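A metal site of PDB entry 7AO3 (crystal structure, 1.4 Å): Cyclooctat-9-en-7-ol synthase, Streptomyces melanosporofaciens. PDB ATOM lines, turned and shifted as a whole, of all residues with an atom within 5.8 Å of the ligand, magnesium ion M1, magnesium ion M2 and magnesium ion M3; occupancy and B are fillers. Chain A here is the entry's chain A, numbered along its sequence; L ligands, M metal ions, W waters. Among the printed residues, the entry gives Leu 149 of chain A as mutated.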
ATOM      1  N   ASN A 103      -6.957  15.075   6.955  1.00  0.00           N
ATOM      2  CA  ASN A 103      -8.125  14.272   6.610  1.00  0.00           C
ATOM      3  C   ASN A 103      -8.283  13.081   7.556  1.00  0.00           C
ATOM      4  O   ASN A 103      -9.415  12.671   7.835  1.00  0.00           O
ATOM      5  CB  ASN A 103      -8.124  13.914   5.119  1.00  0.00           C
ATOM      6  CG  ASN A 103      -9.536  13.722   4.536  1.00  0.00           C
ATOM      7  OD1 ASN A 103      -9.931  12.619   4.207  1.00  0.00           O
ATOM      8  ND2 ASN A 103     -10.275  14.809   4.392  1.00  0.00           N
ATOM      9  N   THR A 106      -9.648  14.594  11.116  1.00  0.00           N
ATOM     10  CA  THR A 106     -11.048  15.008  11.021  1.00  0.00           C
ATOM     11  C   THR A 106     -11.977  13.828  10.744  1.00  0.00           C
ATOM     12  O   THR A 106     -13.169  13.889  11.062  1.00  0.00           O
ATOM     13  CB  THR A 106     -11.257  16.172  10.012  1.00  0.00           C
ATOM     14  OG1 THR A 106     -10.825  15.791   8.693  1.00  0.00           O
ATOM     15  CG2 THR A 106     -10.479  17.385  10.460  1.00  0.00           C
ATOM     16  N   PHE A 107     -11.452  12.718  10.195  1.00  0.00           N
ATOM     17  CA  PHE A 107     -12.259  11.507  10.114  1.00  0.00           C
ATOM     18  C   PHE A 107     -12.574  10.971  11.496  1.00  0.00           C
ATOM     19  O   PHE A 107     -13.694  10.484  11.750  1.00  0.00           O
ATOM     20  CB  PHE A 107     -11.483  10.432   9.341  1.00  0.00           C
ATOM     21  CG  PHE A 107     -12.168   9.963   8.097  1.00  0.00           C
ATOM     22  CD1 PHE A 107     -13.411   9.322   8.167  1.00  0.00           C
ATOM     23  CD2 PHE A 107     -11.546  10.071   6.865  1.00  0.00           C
ATOM     24  CE1 PHE A 107     -14.017   8.873   7.075  1.00  0.00           C
ATOM     25  CE2 PHE A 107     -12.184   9.558   5.728  1.00  0.00           C
ATOM     26  CZ  PHE A 107     -13.426   8.953   5.861  1.00  0.00           C
ATOM     27  N   ASP A 110     -15.371  12.978  12.864  1.00  0.00           N
ATOM     28  CA  ASP A 110     -16.607  12.523  12.217  1.00  0.00           C
ATOM     29  C   ASP A 110     -17.144  11.261  12.879  1.00  0.00           C
ATOM     30  O   ASP A 110     -18.366  11.098  13.026  1.00  0.00           O
ATOM     31  CB  ASP A 110     -16.304  12.234  10.729  1.00  0.00           C
ATOM     32  CG  ASP A 110     -17.553  12.007   9.890  1.00  0.00           C
ATOM     33  OD1 ASP A 110     -18.263  13.000   9.567  1.00  0.00           O
ATOM     34  OD2 ASP A 110     -17.838  10.814   9.563  1.00  0.00           O
ATOM     35  N   ASP A 111     -16.242  10.344  13.254  1.00  0.00           N
ATOM     36  CA  ASP A 111     -16.637   9.065  13.843  1.00  0.00           C
ATOM     37  C   ASP A 111     -16.928   9.145  15.336  1.00  0.00           C
ATOM     38  O   ASP A 111     -17.395   8.151  15.895  1.00  0.00           O
ATOM     39  CB  ASP A 111     -15.566   7.986  13.580  1.00  0.00           C
ATOM     40  CG  ASP A 111     -15.669   7.361  12.210  1.00  0.00           C
ATOM     41  OD1 ASP A 111     -16.750   7.444  11.551  1.00  0.00           O
ATOM     42  OD2 ASP A 111     -14.674   6.755  11.807  1.00  0.00           O
ATOM     43  N   LEU A 149     -15.037  22.970   9.226  1.00  0.00           N
ATOM     44  CA  LEU A 149     -15.579  21.619   9.061  1.00  0.00           C
ATOM     45  C   LEU A 149     -15.908  20.978  10.408  1.00  0.00           C
ATOM     46  O   LEU A 149     -17.027  20.469  10.612  1.00  0.00           O
ATOM     47  CB  LEU A 149     -14.608  20.762   8.246  1.00  0.00           C
ATOM     48  CG  LEU A 149     -15.089  19.297   8.156  1.00  0.00           C
ATOM     49  CD1 LEU A 149     -16.461  19.147   7.455  1.00  0.00           C
ATOM     50  CD2 LEU A 149     -14.021  18.483   7.481  1.00  0.00           C
ATOM     51  N   ASP A 153     -19.563  19.848  11.643  1.00  0.00           N
ATOM     52  CA  ASP A 153     -19.934  18.492  12.051  1.00  0.00           C
ATOM     53  C   ASP A 153     -20.570  18.481  13.429  1.00  0.00           C
ATOM     54  O   ASP A 153     -21.599  17.821  13.656  1.00  0.00           O
ATOM     55  CB  ASP A 153     -18.705  17.577  12.042  1.00  0.00           C
ATOM     56  CG  ASP A 153     -19.007  16.228  12.573  1.00  0.00           C
ATOM     57  OD1 ASP A 153     -19.749  15.456  11.941  1.00  0.00           O
ATOM     58  OD2 ASP A 153     -18.563  15.980  13.694  1.00  0.00           O
ATOM     59  N   ARG A 177     -24.085  19.272   1.727  1.00  0.00           N
ATOM     60  CA  ARG A 177     -22.895  18.414   1.669  1.00  0.00           C
ATOM     61  C   ARG A 177     -21.627  19.099   1.131  1.00  0.00           C
ATOM     62  O   ARG A 177     -20.515  18.595   1.383  1.00  0.00           O
ATOM     63  CB  ARG A 177     -23.189  17.158   0.829  1.00  0.00           C
ATOM     64  CG  ARG A 177     -24.163  16.232   1.547  1.00  0.00           C
ATOM     65  CD  ARG A 177     -23.510  15.600   2.789  1.00  0.00           C
ATOM     66  NE  ARG A 177     -23.309  14.156   2.597  1.00  0.00           N
ATOM     67  CZ  ARG A 177     -22.355  13.427   3.218  1.00  0.00           C
ATOM     68  NH1 ARG A 177     -21.531  13.987   4.101  1.00  0.00           N
ATOM     69  NH2 ARG A 177     -22.172  12.130   2.928  1.00  0.00           N
ATOM     70  N   ASP A 180     -20.449  19.681   4.415  1.00  0.00           N
ATOM     71  CA  ASP A 180     -20.531  18.579   5.377  1.00  0.00           C
ATOM     72  C   ASP A 180     -19.660  17.375   5.012  1.00  0.00           C
ATOM     73  O   ASP A 180     -19.113  16.719   5.913  1.00  0.00           O
ATOM     74  CB  ASP A 180     -21.992  18.145   5.555  1.00  0.00           C
ATOM     75  CG  ASP A 180     -22.139  16.973   6.538  1.00  0.00           C
ATOM     76  OD1 ASP A 180     -22.151  15.800   6.098  1.00  0.00           O
ATOM     77  OD2 ASP A 180     -22.344  17.210   7.740  1.00  0.00           O
ATOM     78  N   ILE A 181     -19.568  17.031   3.719  1.00  0.00           N
ATOM     79  CA  ILE A 181     -18.755  15.873   3.346  1.00  0.00           C
ATOM     80  C   ILE A 181     -17.275  16.178   3.515  1.00  0.00           C
ATOM     81  O   ILE A 181     -16.475  15.245   3.542  1.00  0.00           O
ATOM     82  CB  ILE A 181     -19.093  15.301   1.957  1.00  0.00           C
ATOM     83  CG1 ILE A 181     -18.629  13.832   1.865  1.00  0.00           C
ATOM     84  CG2 ILE A 181     -18.476  16.152   0.787  1.00  0.00           C
ATOM     85  CD1 ILE A 181     -19.200  13.095   0.685  1.00  0.00           C
ATOM     86  N   GLY A 182     -16.907  17.460   3.658  1.00  0.00           N
ATOM     87  CA  GLY A 182     -15.534  17.832   3.833  1.00  0.00           C
ATOM     88  C   GLY A 182     -14.819  18.239   2.549  1.00  0.00           C
ATOM     89  O   GLY A 182     -13.602  18.436   2.579  1.00  0.00           O
ATOM     90  N   ASN A 220     -20.215   8.022  -1.917  1.00  0.00           N
ATOM     91  CA  ASN A 220     -20.071   7.752  -0.494  1.00  0.00           C
ATOM     92  C   ASN A 220     -21.383   7.321   0.126  1.00  0.00           C
ATOM     93  O   ASN A 220     -21.426   6.408   0.967  1.00  0.00           O
ATOM     94  CB  ASN A 220     -19.582   8.990   0.266  1.00  0.00           C
ATOM     95  CG  ASN A 220     -19.549   8.729   1.753  1.00  0.00           C
ATOM     96  OD1 ASN A 220     -20.504   9.054   2.496  1.00  0.00           O
ATOM     97  ND2 ASN A 220     -18.500   8.027   2.193  1.00  0.00           N
ATOM     98  N   ASP A 221     -22.468   7.995  -0.269  1.00  0.00           N
ATOM     99  CA  ASP A 221     -23.763   7.728   0.342  1.00  0.00           C
ATOM    100  C   ASP A 221     -24.224   6.298   0.033  1.00  0.00           C
ATOM    101  O   ASP A 221     -24.767   5.600   0.917  1.00  0.00           O
ATOM    102  CB  ASP A 221     -24.816   8.712  -0.177  1.00  0.00           C
ATOM    103  CG  ASP A 221     -24.687  10.106   0.410  1.00  0.00           C
ATOM    104  OD1 ASP A 221     -23.819  10.338   1.284  1.00  0.00           O
ATOM    105  OD2 ASP A 221     -25.517  10.966  -0.005  1.00  0.00           O
ATOM    106  N   SER A 224     -21.989   3.936   2.265  1.00  0.00           N
ATOM    107  CA  SER A 224     -22.049   4.165   3.694  1.00  0.00           C
ATOM    108  C   SER A 224     -23.477   4.172   4.238  1.00  0.00           C
ATOM    109  O   SER A 224     -23.657   4.314   5.445  1.00  0.00           O
ATOM    110  CB  SER A 224     -21.291   5.436   4.103  1.00  0.00           C
ATOM    111  OG  SER A 224     -21.850   6.640   3.581  1.00  0.00           O
ATOM    112  N   ARG A 227     -24.205   1.521   7.252  1.00  0.00           N
ATOM    113  CA  ARG A 227     -23.640   1.980   8.509  1.00  0.00           C
ATOM    114  C   ARG A 227     -24.444   3.148   9.069  1.00  0.00           C
ATOM    115  O   ARG A 227     -24.824   3.163  10.245  1.00  0.00           O
ATOM    116  CB  ARG A 227     -22.179   2.400   8.302  1.00  0.00           C
ATOM    117  CG  ARG A 227     -21.641   3.258   9.440  1.00  0.00           C
ATOM    118  CD  ARG A 227     -20.121   3.370   9.455  1.00  0.00           C
ATOM    119  NE  ARG A 227     -19.564   3.652   8.146  1.00  0.00           N
ATOM    120  CZ  ARG A 227     -19.396   4.870   7.636  1.00  0.00           C
ATOM    121  NH1 ARG A 227     -19.758   5.968   8.342  1.00  0.00           N
ATOM    122  NH2 ARG A 227     -18.861   4.973   6.420  1.00  0.00           N
ATOM    123  N   GLU A 228     -24.732   4.147   8.217  1.00  0.00           N
ATOM    124  CA  GLU A 228     -25.354   5.390   8.678  1.00  0.00           C
ATOM    125  C   GLU A 228     -26.765   5.143   9.187  1.00  0.00           C
ATOM    126  O   GLU A 228     -27.138   5.613  10.269  1.00  0.00           O
ATOM    127  CB  GLU A 228     -25.275   6.444   7.567  1.00  0.00           C
ATOM    128  CG  GLU A 228     -23.830   6.889   7.450  1.00  0.00           C
ATOM    129  CD  GLU A 228     -23.525   7.733   6.246  1.00  0.00           C
ATOM    130  OE1 GLU A 228     -24.446   8.015   5.453  1.00  0.00           O
ATOM    131  OE2 GLU A 228     -22.334   8.074   6.083  1.00  0.00           O
ATOM    132  N   GLN A 233     -27.872   8.109  11.545  1.00  0.00           N
ATOM    133  CA  GLN A 233     -27.336   9.277  10.849  1.00  0.00           C
ATOM    134  C   GLN A 233     -28.171   9.527   9.598  1.00  0.00           C
ATOM    135  O   GLN A 233     -28.335   8.624   8.775  1.00  0.00           O
ATOM    136  CB  GLN A 233     -25.878   8.979  10.472  1.00  0.00           C
ATOM    137  CG  GLN A 233     -24.980   9.057  11.717  1.00  0.00           C
ATOM    138  CD  GLN A 233     -23.587   8.503  11.501  1.00  0.00           C
ATOM    139  OE1 GLN A 233     -23.399   7.431  10.893  1.00  0.00           O
ATOM    140  NE2 GLN A 233     -22.593   9.242  11.989  1.00  0.00           N
ATOM    141  N   THR A 235     -27.638  11.936   7.184  1.00  0.00           N
ATOM    142  CA  THR A 235     -26.987  12.688   6.091  1.00  0.00           C
ATOM    143  C   THR A 235     -26.638  11.681   4.989  1.00  0.00           C
ATOM    144  O   THR A 235     -25.507  11.208   4.858  1.00  0.00           O
ATOM    145  CB  THR A 235     -25.770  13.452   6.608  1.00  0.00           C
ATOM    146  OG1 THR A 235     -26.182  14.271   7.706  1.00  0.00           O
ATOM    147  CG2 THR A 235     -25.193  14.401   5.544  1.00  0.00           C
ATOM    148  N   ASN A 236     -27.637  11.346   4.164  1.00  0.00           N
ATOM    149  CA  ASN A 236     -27.446  10.360   3.105  1.00  0.00           C
ATOM    150  C   ASN A 236     -28.562  10.547   2.081  1.00  0.00           C
ATOM    151  O   ASN A 236     -29.744  10.473   2.432  1.00  0.00           O
ATOM    152  CB  ASN A 236     -27.481   8.927   3.723  1.00  0.00           C
ATOM    153  CG  ASN A 236     -26.988   7.899   2.748  1.00  0.00           C
ATOM    154  OD1 ASN A 236     -27.582   7.754   1.666  1.00  0.00           O
ATOM    155  ND2 ASN A 236     -25.889   7.206   3.074  1.00  0.00           N
ATOM    156  N   TRP A 288     -11.179   3.847  -3.712  1.00  0.00           N
ATOM    157  CA  TRP A 288     -10.932   3.607  -2.290  1.00  0.00           C
ATOM    158  C   TRP A 288     -12.188   3.121  -1.583  1.00  0.00           C
ATOM    159  O   TRP A 288     -12.142   2.162  -0.793  1.00  0.00           O
ATOM    160  CB  TRP A 288     -10.426   4.916  -1.658  1.00  0.00           C
ATOM    161  CG  TRP A 288     -10.398   4.905  -0.149  1.00  0.00           C
ATOM    162  CD1 TRP A 288      -9.515   4.244   0.668  1.00  0.00           C
ATOM    163  CD2 TRP A 288     -11.295   5.601   0.716  1.00  0.00           C
ATOM    164  NE1 TRP A 288      -9.806   4.496   1.994  1.00  0.00           N
ATOM    165  CE2 TRP A 288     -10.892   5.348   2.045  1.00  0.00           C
ATOM    166  CE3 TRP A 288     -12.399   6.433   0.479  1.00  0.00           C
ATOM    167  CZ2 TRP A 288     -11.549   5.899   3.144  1.00  0.00           C
ATOM    168  CZ3 TRP A 288     -13.066   6.980   1.570  1.00  0.00           C
ATOM    169  CH2 TRP A 288     -12.626   6.708   2.898  1.00  0.00           C
ATOM    170  N   ARG A 294     -13.491   0.090   5.451  1.00  0.00           N
ATOM    171  CA  ARG A 294     -14.447   1.013   6.074  1.00  0.00           C
ATOM    172  C   ARG A 294     -15.861   0.828   5.525  1.00  0.00           C
ATOM    173  O   ARG A 294     -16.834   1.041   6.240  1.00  0.00           O
ATOM    174  CB  ARG A 294     -13.988   2.467   5.840  1.00  0.00           C
ATOM    175  CG  ARG A 294     -15.044   3.516   6.311  1.00  0.00           C
ATOM    176  CD  ARG A 294     -14.502   4.943   6.332  1.00  0.00           C
ATOM    177  NE  ARG A 294     -15.425   5.908   6.951  1.00  0.00           N
ATOM    178  CZ  ARG A 294     -15.559   6.079   8.264  1.00  0.00           C
ATOM    179  NH1 ARG A 294     -14.803   5.350   9.094  1.00  0.00           N
ATOM    180  NH2 ARG A 294     -16.443   6.961   8.734  1.00  0.00           N
ATOM    181  N   TYR A 295     -15.994   0.475   4.245  1.00  0.00           N
ATOM    182  CA  TYR A 295     -17.294   0.340   3.590  1.00  0.00           C
ATOM    183  C   TYR A 295     -17.671  -1.114   3.307  1.00  0.00           C
ATOM    184  O   TYR A 295     -18.668  -1.372   2.630  1.00  0.00           O
ATOM    185  CB  TYR A 295     -17.323   1.185   2.290  1.00  0.00           C
ATOM    186  CG  TYR A 295     -16.950   2.626   2.573  1.00  0.00           C
ATOM    187  CD1 TYR A 295     -17.885   3.515   3.128  1.00  0.00           C
ATOM    188  CD2 TYR A 295     -15.656   3.085   2.365  1.00  0.00           C
ATOM    189  CE1 TYR A 295     -17.532   4.872   3.453  1.00  0.00           C
ATOM    190  CE2 TYR A 295     -15.295   4.412   2.648  1.00  0.00           C
ATOM    191  CZ  TYR A 295     -16.240   5.303   3.202  1.00  0.00           C
ATOM    192  OH  TYR A 295     -15.910   6.586   3.547  1.00  0.00           O
HETATM  193  C1  LIG L   1     -16.331  12.147   5.704  1.00  0.00           C
HETATM  194  C2  LIG L   1     -14.925  12.416   6.186  1.00  0.00           C
HETATM  195  C3  LIG L   1     -16.793  10.765   6.108  1.00  0.00           C
HETATM  196  C4  LIG L   1     -18.026  10.237   5.362  1.00  0.00           C
HETATM  197  O1  LIG L   1     -18.568   8.520   7.382  1.00  0.00           O
HETATM  198  P1  LIG L   1     -18.311   8.472   5.890  1.00  0.00           P
HETATM  199  O2  LIG L   1     -19.444   7.865   5.096  1.00  0.00           O
HETATM  200  O3  LIG L   1     -17.040   7.689   5.634  1.00  0.00           O
HETATM  201  P2  LIG L   1     -19.568  11.213   5.707  1.00  0.00           P
HETATM  202  O4  LIG L   1     -19.381  12.605   5.038  1.00  0.00           O
HETATM  203  O5  LIG L   1     -20.792  10.466   5.203  1.00  0.00           O
HETATM  204  O6  LIG L   1     -19.633  11.405   7.242  1.00  0.00           O
HETATM  205  O7  LIG L   1     -17.856  10.256   3.958  1.00  0.00           O
HETATM  206  N1  LIG L   1     -14.428  13.710   5.653  1.00  0.00           N
HETATM  207 MG    MG M   1     -21.224   8.646   4.414  1.00  0.00          MG
HETATM  208 MG    MG M   2     -19.386   9.900   8.706  1.00  0.00          MG
HETATM  209 MG    MG M   3     -20.013  13.097   8.397  1.00  0.00          MG
HETATM  210  O   HOH W   1     -21.857  13.468   7.408  1.00  0.00           O
HETATM  211  O   HOH W   2     -20.738  11.621   9.659  1.00  0.00           O
HETATM  212  O   HOH W   3     -23.025  11.303   6.300  1.00  0.00           O
HETATM  213  O   HOH W   4     -19.177   8.688  10.437  1.00  0.00           O
HETATM  214  O   HOH W   5     -12.086  13.919   7.045  1.00  0.00           O
HETATM  215  O   HOH W   6     -20.521  14.810   9.533  1.00  0.00           O
HETATM  216  O   HOH W   7     -15.429   9.349   2.902  1.00  0.00           O
HETATM  217  O   HOH W   8     -16.067  15.622   6.656  1.00  0.00           O
HETATM  218  O   HOH W   9     -23.061   9.364   3.632  1.00  0.00           O
HETATM  219  O   HOH W  10     -21.256   8.951   8.349  1.00  0.00           O
HETATM  220  O   HOH W  11     -18.942  14.221   6.938  1.00  0.00           O
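Water W4 lies within hydrogen-bond range of OD1 of Asp 111 (2.9 Å) and NH1 of Arg 227 (3.5 Å). Water W1 bridges OD1 of Asp 180 and NH1 of Arg 177. Water W11 bridges an oxygen (O4) of the ligand and the backbone carbonyl oxygen (O) of Asp 180. Water W8 lies within hydrogen-bond range of N1 of the ligand (2.7 Å), O of Ile 181 (3.2 Å) and O of Asp 180 (3.3 Å). Water W5 lies within hydrogen-bond range of N1 of the ligand, OG1 of Thr 106, O of Asn 103 and N of Phe 107. Water W7 lies within hydrogen-bond range of an oxygen (O7) of the ligand (2.8 Å), the side-chain hydroxyl of Tyr 295 (2.9 Å) and the side-chain amide nitrogen of Asn 220 (3.4 Å).
Arg 227 touches magnesium ion M2. Two residues have an atom within 4 Å of magnesium ion M2: Asp 110 and Arg 227. The nearest printed residue that does not touch magnesium ion M2 is Arg 294 (4.2 Å).
OH of Tyr 295 sits at hydrogen-bond distance from O3 of the ligand (2.6 Å). The guanidinium group (NH1) of Arg 177 lies within salt-bridge range of an oxygen (O4) of the ligand, 2.7 Å away. The guanidinium group (NE) of Arg 294 is in salt-bridge range of an oxygen (O3) of the ligand (2.7 Å). An oxygen (O3) of the ligand is in salt-bridge range of the guanidinium group of Arg 227, 3.4 Å away. N1 of the ligand is in hydrogen-bond range of O of Ile 181.
Magnesium ion M2 is bound by OD2 of Asp 110 (2.0 Å), O1 of the ligand (2.1 Å), O6 of the ligand (2.1 Å), water W4 (2.1 Å), water W10 (2.1 Å) and water W2 (2.4 Å).
O of Glu 228 sits at hydrogen-bond distance from N of Gln 233, 2.9 Å away. The side-chain amide nitrogen of Asn 236 is in hydrogen-bond range of the side-chain carboxylate of Glu 228 (2.9 Å). The side-chain hydroxyl (OH) of Tyr 295 lies within hydrogen-bond range of the side-chain amide nitrogen (ND2) of Asn 220, at 3.3 Å. OD1 of Asp 180 lies within salt-bridge range of NH1 of Arg 177 (2.8 Å). OD1 of Asp 221 lies within salt-bridge range of NH2 of Arg 177, at 2.9 Å. The guanidinium group of Arg 294 lies within salt-bridge range of the side-chain carboxylate of Asp 111, at 2.9 Å.
Magnesium ion M3 is bound by water W2 (2.1 Å), O6 of the ligand (2.1 Å), OD1 of Asp 110 (2.1 Å), water W6 (2.1 Å), water W1 (2.1 Å) and water W11 (2.1 Å).
Phe 107 touches the ligand (CE1 to C3, 3.5 Å). Hydrophobic or aromatic side chains that line the ligand: Phe 107, Ile 181 and Tyr 295. The nearest printed residue that does not touch the ligand is Asp 180 (4.2 Å).
Magnesium ion M1 is bound by O5 of the ligand (2.0 Å), O2 of the ligand (2.1 Å), OE2 of Glu 228 (2.1 Å), OD1 of Asn 220 (2.1 Å), water W9 (2.1 Å) and OG of Ser 224 (2.3 Å). Magnesium ion M1 has six donor atoms within binding distance.
Within 4 Å of magnesium ion M3: Asp 110.
Merely in contact with magnesium ion M1: Arg 177 (3.9 Å). Of the 22 residues printed, 4 come within 4 Å of magnesium ion M1. The nearest printed residue that does not touch magnesium ion M1 is Asp 221 (4.4 Å).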
